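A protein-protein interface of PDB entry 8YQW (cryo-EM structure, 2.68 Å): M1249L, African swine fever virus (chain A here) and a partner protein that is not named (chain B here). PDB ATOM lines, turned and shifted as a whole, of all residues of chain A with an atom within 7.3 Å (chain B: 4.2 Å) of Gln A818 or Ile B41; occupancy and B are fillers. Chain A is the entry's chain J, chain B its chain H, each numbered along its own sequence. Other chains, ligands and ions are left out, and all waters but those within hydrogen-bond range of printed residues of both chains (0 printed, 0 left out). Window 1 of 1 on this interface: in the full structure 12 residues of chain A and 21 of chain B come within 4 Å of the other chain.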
ATOM      1  N   LYS A 813       8.836  -3.047   4.898  1.00  0.00           N
ATOM      2  CA  LYS A 813       9.705  -2.463   3.878  1.00  0.00           C
ATOM      3  C   LYS A 813       8.931  -1.513   2.969  1.00  0.00           C
ATOM      4  O   LYS A 813       9.464  -0.486   2.530  1.00  0.00           O
ATOM      5  CB  LYS A 813      10.375  -3.570   3.066  1.00  0.00           C
ATOM      6  CG  LYS A 813      11.451  -3.065   2.124  1.00  0.00           C
ATOM      7  CD  LYS A 813      12.277  -4.206   1.558  1.00  0.00           C
ATOM      8  CE  LYS A 813      13.387  -3.682   0.669  1.00  0.00           C
ATOM      9  NZ  LYS A 813      14.284  -4.771   0.203  1.00  0.00           N
ATOM     10  N   ALA A 814       7.671  -1.840   2.675  1.00  0.00           N
ATOM     11  CA  ALA A 814       6.823  -0.944   1.898  1.00  0.00           C
ATOM     12  C   ALA A 814       6.577   0.358   2.642  1.00  0.00           C
ATOM     13  O   ALA A 814       6.487   1.426   2.026  1.00  0.00           O
ATOM     14  CB  ALA A 814       5.500  -1.632   1.565  1.00  0.00           C
ATOM     15  N   LEU A 815       6.443   0.288   3.968  1.00  0.00           N
ATOM     16  CA  LEU A 815       6.387   1.518   4.755  1.00  0.00           C
ATOM     17  C   LEU A 815       7.665   2.322   4.588  1.00  0.00           C
ATOM     18  O   LEU A 815       7.625   3.549   4.444  1.00  0.00           O
ATOM     19  CB  LEU A 815       6.147   1.197   6.231  1.00  0.00           C
ATOM     20  CG  LEU A 815       5.687   2.346   7.138  1.00  0.00           C
ATOM     21  CD1 LEU A 815       4.821   1.804   8.260  1.00  0.00           C
ATOM     22  CD2 LEU A 815       6.860   3.127   7.710  1.00  0.00           C
ATOM     23  N   LEU A 816       8.811   1.643   4.609  1.00  0.00           N
ATOM     24  CA  LEU A 816      10.080   2.336   4.408  1.00  0.00           C
ATOM     25  C   LEU A 816      10.200   2.947   3.018  1.00  0.00           C
ATOM     26  O   LEU A 816      10.930   3.929   2.846  1.00  0.00           O
ATOM     27  CB  LEU A 816      11.249   1.387   4.648  1.00  0.00           C
ATOM     28  CG  LEU A 816      11.478   0.979   6.098  1.00  0.00           C
ATOM     29  CD1 LEU A 816      12.585  -0.054   6.180  1.00  0.00           C
ATOM     30  CD2 LEU A 816      11.805   2.198   6.938  1.00  0.00           C
ATOM     31  N   ALA A 817       9.500   2.402   2.026  1.00  0.00           N
ATOM     32  CA  ALA A 817       9.641   2.822   0.632  1.00  0.00           C
ATOM     33  C   ALA A 817       8.567   3.813   0.197  1.00  0.00           C
ATOM     34  O   ALA A 817       8.153   3.801  -0.965  1.00  0.00           O
ATOM     35  CB  ALA A 817       9.634   1.602  -0.282  1.00  0.00           C
ATOM     36  N   GLN A 818       8.102   4.688   1.084  1.00  0.00           N
ATOM     37  CA  GLN A 818       7.034   5.631   0.769  1.00  0.00           C
ATOM     38  C   GLN A 818       7.606   7.038   0.650  1.00  0.00           C
ATOM     39  O   GLN A 818       8.235   7.540   1.587  1.00  0.00           O
ATOM     40  CB  GLN A 818       5.934   5.588   1.830  1.00  0.00           C
ATOM     41  CG  GLN A 818       5.074   4.339   1.773  1.00  0.00           C
ATOM     42  CD  GLN A 818       4.452   4.124   0.409  1.00  0.00           C
ATOM     43  OE1 GLN A 818       3.972   5.063  -0.222  1.00  0.00           O
ATOM     44  NE2 GLN A 818       4.465   2.883  -0.057  1.00  0.00           N
ATOM     45  N   GLN A 819       7.380   7.672  -0.502  1.00  0.00           N
ATOM     46  CA  GLN A 819       7.856   9.029  -0.742  1.00  0.00           C
ATOM     47  C   GLN A 819       6.977  10.088  -0.093  1.00  0.00           C
ATOM     48  O   GLN A 819       7.426  11.227   0.073  1.00  0.00           O
ATOM     49  CB  GLN A 819       7.929   9.306  -2.246  1.00  0.00           C
ATOM     50  CG  GLN A 819       8.766   8.322  -3.050  1.00  0.00           C
ATOM     51  CD  GLN A 819      10.232   8.377  -2.699  1.00  0.00           C
ATOM     52  OE1 GLN A 819      10.756   9.428  -2.346  1.00  0.00           O
ATOM     53  NE2 GLN A 819      10.907   7.241  -2.799  1.00  0.00           N
ATOM     54  N   GLY A 820       5.752   9.745   0.272  1.00  0.00           N
ATOM     55  CA  GLY A 820       4.773  10.703   0.742  1.00  0.00           C
ATOM     56  C   GLY A 820       3.679  10.936  -0.285  1.00  0.00           C
ATOM     57  O   GLY A 820       3.760  10.522  -1.441  1.00  0.00           O
ATOM     58  N   PHE A 821       2.629  11.618   0.169  1.00  0.00           N
ATOM     59  CA  PHE A 821       1.484  11.891  -0.688  1.00  0.00           C
ATOM     60  C   PHE A 821       0.706  13.070  -0.121  1.00  0.00           C
ATOM     61  O   PHE A 821       0.621  13.246   1.095  1.00  0.00           O
ATOM     62  CB  PHE A 821       0.577  10.663  -0.817  1.00  0.00           C
ATOM     63  CG  PHE A 821      -0.533  10.835  -1.808  1.00  0.00           C
ATOM     64  CD1 PHE A 821      -0.261  11.231  -3.106  1.00  0.00           C
ATOM     65  CD2 PHE A 821      -1.847  10.608  -1.445  1.00  0.00           C
ATOM     66  CE1 PHE A 821      -1.277  11.392  -4.019  1.00  0.00           C
ATOM     67  CE2 PHE A 821      -2.866  10.772  -2.354  1.00  0.00           C
ATOM     68  CZ  PHE A 821      -2.580  11.164  -3.643  1.00  0.00           C
ATOM     69  N   TYR A 822       0.137  13.868  -1.020  1.00  0.00           N
ATOM     70  CA  TYR A 822      -0.596  15.067  -0.647  1.00  0.00           C
ATOM     71  C   TYR A 822      -1.873  15.164  -1.467  1.00  0.00           C
ATOM     72  O   TYR A 822      -1.930  14.716  -2.613  1.00  0.00           O
ATOM     73  CB  TYR A 822       0.259  16.322  -0.852  1.00  0.00           C
ATOM     74  CG  TYR A 822      -0.385  17.617  -0.407  1.00  0.00           C
ATOM     75  CD1 TYR A 822      -0.341  18.018   0.917  1.00  0.00           C
ATOM     76  CD2 TYR A 822      -1.019  18.445  -1.322  1.00  0.00           C
ATOM     77  CE1 TYR A 822      -0.920  19.199   1.321  1.00  0.00           C
ATOM     78  CE2 TYR A 822      -1.600  19.628  -0.926  1.00  0.00           C
ATOM     79  CZ  TYR A 822      -1.550  20.000   0.396  1.00  0.00           C
ATOM     80  OH  TYR A 822      -2.132  21.181   0.792  1.00  0.00           O
ATOM     81  N   ASN A 823      -2.899  15.756  -0.861  1.00  0.00           N
ATOM     82  CA  ASN A 823      -4.180  15.995  -1.513  1.00  0.00           C
ATOM     83  C   ASN A 823      -4.532  17.462  -1.347  1.00  0.00           C
ATOM     84  O   ASN A 823      -4.502  17.983  -0.229  1.00  0.00           O
ATOM     85  CB  ASN A 823      -5.279  15.112  -0.917  1.00  0.00           C
ATOM     86  CG  ASN A 823      -5.114  13.657  -1.278  1.00  0.00           C
ATOM     87  OD1 ASN A 823      -4.507  12.887  -0.536  1.00  0.00           O
ATOM     88  ND2 ASN A 823      -5.661  13.267  -2.422  1.00  0.00           N
ATOM     89  N   ILE B  29       6.383  10.409   8.271  1.00  0.00           N
ATOM     90  CA  ILE B  29       5.240   9.724   7.680  1.00  0.00           C
ATOM     91  C   ILE B  29       4.556   8.855   8.723  1.00  0.00           C
ATOM     92  O   ILE B  29       3.322   8.768   8.766  1.00  0.00           O
ATOM     93  CB  ILE B  29       5.679   8.915   6.446  1.00  0.00           C
ATOM     94  CG1 ILE B  29       6.089   9.863   5.318  1.00  0.00           C
ATOM     95  CG2 ILE B  29       4.562   8.002   5.976  1.00  0.00           C
ATOM     96  CD1 ILE B  29       6.736   9.175   4.146  1.00  0.00           C
ATOM     97  N   MET B  33       0.556   8.778   8.997  1.00  0.00           N
ATOM     98  CA  MET B  33       0.079   7.674   8.171  1.00  0.00           C
ATOM     99  C   MET B  33      -1.369   7.307   8.469  1.00  0.00           C
ATOM    100  O   MET B  33      -2.255   7.573   7.650  1.00  0.00           O
ATOM    101  CB  MET B  33       1.004   6.472   8.375  1.00  0.00           C
ATOM    102  CG  MET B  33       0.587   5.195   7.692  1.00  0.00           C
ATOM    103  SD  MET B  33       1.883   3.956   7.847  1.00  0.00           S
ATOM    104  CE  MET B  33       1.934   3.747   9.623  1.00  0.00           C
ATOM    105  N   LEU B  37      -2.696   0.879   5.401  1.00  0.00           N
ATOM    106  CA  LEU B  37      -1.549   0.051   5.083  1.00  0.00           C
ATOM    107  C   LEU B  37      -0.504   0.871   4.331  1.00  0.00           C
ATOM    108  O   LEU B  37      -0.846   1.794   3.587  1.00  0.00           O
ATOM    109  CB  LEU B  37      -1.959  -1.156   4.246  1.00  0.00           C
ATOM    110  CG  LEU B  37      -2.874  -2.178   4.922  1.00  0.00           C
ATOM    111  CD1 LEU B  37      -3.227  -3.296   3.956  1.00  0.00           C
ATOM    112  CD2 LEU B  37      -2.247  -2.724   6.185  1.00  0.00           C
ATOM    113  N   PRO B  38       0.779   0.566   4.529  1.00  0.00           N
ATOM    114  CA  PRO B  38       1.830   1.387   3.901  1.00  0.00           C
ATOM    115  C   PRO B  38       1.722   1.482   2.389  1.00  0.00           C
ATOM    116  O   PRO B  38       1.808   2.583   1.832  1.00  0.00           O
ATOM    117  CB  PRO B  38       3.110   0.672   4.339  1.00  0.00           C
ATOM    118  CG  PRO B  38       2.749   0.008   5.617  1.00  0.00           C
ATOM    119  CD  PRO B  38       1.337  -0.442   5.445  1.00  0.00           C
ATOM    120  N   GLN B  39       1.502   0.362   1.706  1.00  0.00           N
ATOM    121  CA  GLN B  39       1.470   0.356   0.248  1.00  0.00           C
ATOM    122  C   GLN B  39       0.269   1.123  -0.288  1.00  0.00           C
ATOM    123  O   GLN B  39       0.192   1.406  -1.487  1.00  0.00           O
ATOM    124  CB  GLN B  39       1.467  -1.081  -0.274  1.00  0.00           C
ATOM    125  CG  GLN B  39       0.140  -1.794  -0.130  1.00  0.00           C
ATOM    126  CD  GLN B  39       0.188  -2.895   0.909  1.00  0.00           C
ATOM    127  OE1 GLN B  39       0.965  -2.832   1.860  1.00  0.00           O
ATOM    128  NE2 GLN B  39      -0.643  -3.913   0.729  1.00  0.00           N
ATOM    129  N   ASN B  40      -0.673   1.464   0.589  1.00  0.00           N
ATOM    130  CA  ASN B  40      -1.848   2.238   0.215  1.00  0.00           C
ATOM    131  C   ASN B  40      -1.697   3.722   0.526  1.00  0.00           C
ATOM    132  O   ASN B  40      -2.659   4.476   0.358  1.00  0.00           O
ATOM    133  CB  ASN B  40      -3.089   1.680   0.912  1.00  0.00           C
ATOM    134  CG  ASN B  40      -3.527   0.350   0.339  1.00  0.00           C
ATOM    135  OD1 ASN B  40      -3.350  -0.696   0.960  1.00  0.00           O
ATOM    136  ND2 ASN B  40      -4.101   0.383  -0.855  1.00  0.00           N
ATOM    137  N   ILE B  41      -0.519   4.157   0.985  1.00  0.00           N
ATOM    138  CA  ILE B  41      -0.313   5.580   1.271  1.00  0.00           C
ATOM    139  C   ILE B  41      -0.571   6.463   0.054  1.00  0.00           C
ATOM    140  O   ILE B  41      -1.228   7.506   0.205  1.00  0.00           O
ATOM    141  CB  ILE B  41       1.082   5.801   1.881  1.00  0.00           C
ATOM    142  CG1 ILE B  41       1.145   5.222   3.292  1.00  0.00           C
ATOM    143  CG2 ILE B  41       1.440   7.278   1.902  1.00  0.00           C
ATOM    144  CD1 ILE B  41       0.201   5.885   4.247  1.00  0.00           C
ATOM    145  N   PRO B  42      -0.110   6.121  -1.166  1.00  0.00           N
ATOM    146  CA  PRO B  42      -0.387   7.001  -2.314  1.00  0.00           C
ATOM    147  C   PRO B  42      -1.826   6.952  -2.807  1.00  0.00           C
ATOM    148  O   PRO B  42      -2.129   7.478  -3.882  1.00  0.00           O
ATOM    149  CB  PRO B  42       0.580   6.487  -3.388  1.00  0.00           C
ATOM    150  CG  PRO B  42       0.889   5.104  -2.990  1.00  0.00           C
ATOM    151  CD  PRO B  42       0.900   5.103  -1.508  1.00  0.00           C
ATOM    152  N   LEU B  43      -2.722   6.329  -2.038  1.00  0.00           N
ATOM    153  CA  LEU B  43      -4.126   6.218  -2.416  1.00  0.00           C
ATOM    154  C   LEU B  43      -5.077   6.744  -1.346  1.00  0.00           C
ATOM    155  O   LEU B  43      -6.295   6.647  -1.522  1.00  0.00           O
ATOM    156  CB  LEU B  43      -4.478   4.760  -2.731  1.00  0.00           C
ATOM    157  CG  LEU B  43      -3.972   4.154  -4.039  1.00  0.00           C
ATOM    158  CD1 LEU B  43      -4.111   2.645  -4.007  1.00  0.00           C
ATOM    159  CD2 LEU B  43      -4.729   4.731  -5.218  1.00  0.00           C
ATOM    160  N   ASP B  44      -4.558   7.306  -0.250  1.00  0.00           N
ATOM    161  CA  ASP B  44      -5.391   7.561   0.923  1.00  0.00           C
ATOM    162  C   ASP B  44      -6.438   8.640   0.675  1.00  0.00           C
ATOM    163  O   ASP B  44      -7.548   8.551   1.211  1.00  0.00           O
ATOM    164  CB  ASP B  44      -4.517   7.939   2.117  1.00  0.00           C
ATOM    165  CG  ASP B  44      -5.258   7.841   3.440  1.00  0.00           C
ATOM    166  OD1 ASP B  44      -6.444   7.453   3.443  1.00  0.00           O
ATOM    167  OD2 ASP B  44      -4.653   8.151   4.485  1.00  0.00           O
ATOM    168  N   LEU B  47      -4.472  12.475   3.015  1.00  0.00           N
ATOM    169  CA  LEU B  47      -3.154  12.764   3.553  1.00  0.00           C
ATOM    170  C   LEU B  47      -2.694  14.161   3.155  1.00  0.00           C
ATOM    171  O   LEU B  47      -3.038  14.672   2.087  1.00  0.00           O
ATOM    172  CB  LEU B  47      -2.143  11.727   3.068  1.00  0.00           C
ATOM    173  CG  LEU B  47      -2.299  10.330   3.664  1.00  0.00           C
ATOM    174  CD1 LEU B  47      -1.269   9.385   3.078  1.00  0.00           C
ATOM    175  CD2 LEU B  47      -2.185  10.378   5.177  1.00  0.00           C
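O of Leu B47 sits at hydrogen-bond distance from N of Asn A823 (3.1 Å). The backbone carbonyl oxygen (O) of Pro B38 sits at hydrogen-bond distance from the side-chain amide nitrogen (NE2) of Gln A818.
The backbone carbonyl oxygen of Ala A814 sits close to the side-chain amide nitrogen of Gln A818 (3.2 Å).
Ala A814 touches Pro B38. CD1 of Leu A815 touches SD of Met B33 (3.7 Å). Gln A818 touches Ile B29 (O to CD1, 3.4 Å). NE2 of Gln A818 touches CA of Gln B39, at 3.9 Å. Gln A818 touches Ile B41. OE1 of Gln A818 touches CD of Pro B42 (3.3 Å). O of Ile B41 touches CD2 of Phe A821 (3.6 Å). Pro B42 touches Phe A821 (O to CE2, 3.7 Å). O of Phe A821 touches CB of Leu B47, 3.7 Å away. CA of Tyr A822 touches O of Leu B47 (3.7 Å).
Of the printed residues of chain B, Ala A814 touches Pro B38. Of the printed residues of chain B, Leu A815 touches Met B33 (3.7 Å) and Pro B38 (3.4 Å). Of the printed residues of chain B, Phe A821 touches Ile B41 (3.6 Å), Pro B42 (3.7 Å) and Leu B47 (3.7 Å). Ile B41 touches just these residues of chain A: Gln A818 (3.6 Å) and Phe A821 (3.6 Å). Printed residues of chain A within 4 Å of Pro B42: Gln A818 (3.3 Å) and Phe A821 (3.7 Å). Asp B44 touches none of the printed residues of chain A. Printed residues of chain A within 4 Å of Leu B47: Phe A821 (3.7 Å), Tyr A822 (3.7 Å) and Asn A823 (3.1 Å). The nearest printed residue of chain B that does not touch Tyr A822 is Ile B41 (6.6 Å).
Of the 11 printed residues of chain A, 6 touch a printed residue of chain B. Printed residues of chain A that touch a printed residue of chain B: Ala A814, Leu A815, Gln A818, Phe A821, Tyr A822 and Asn A823. Hydrophobic or aromatic side chains of chain A within 4 Å of the printed part of chain B: Leu A815 and Phe A821. Printed residues of chain B that touch a printed residue of chain A: Ile B29, Met B33, Pro B38, Gln B39, Ile B41, Pro B42 and Leu B47. Along chain B the printed residues that touch a printed residue of chain A span positions 29 to 47.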
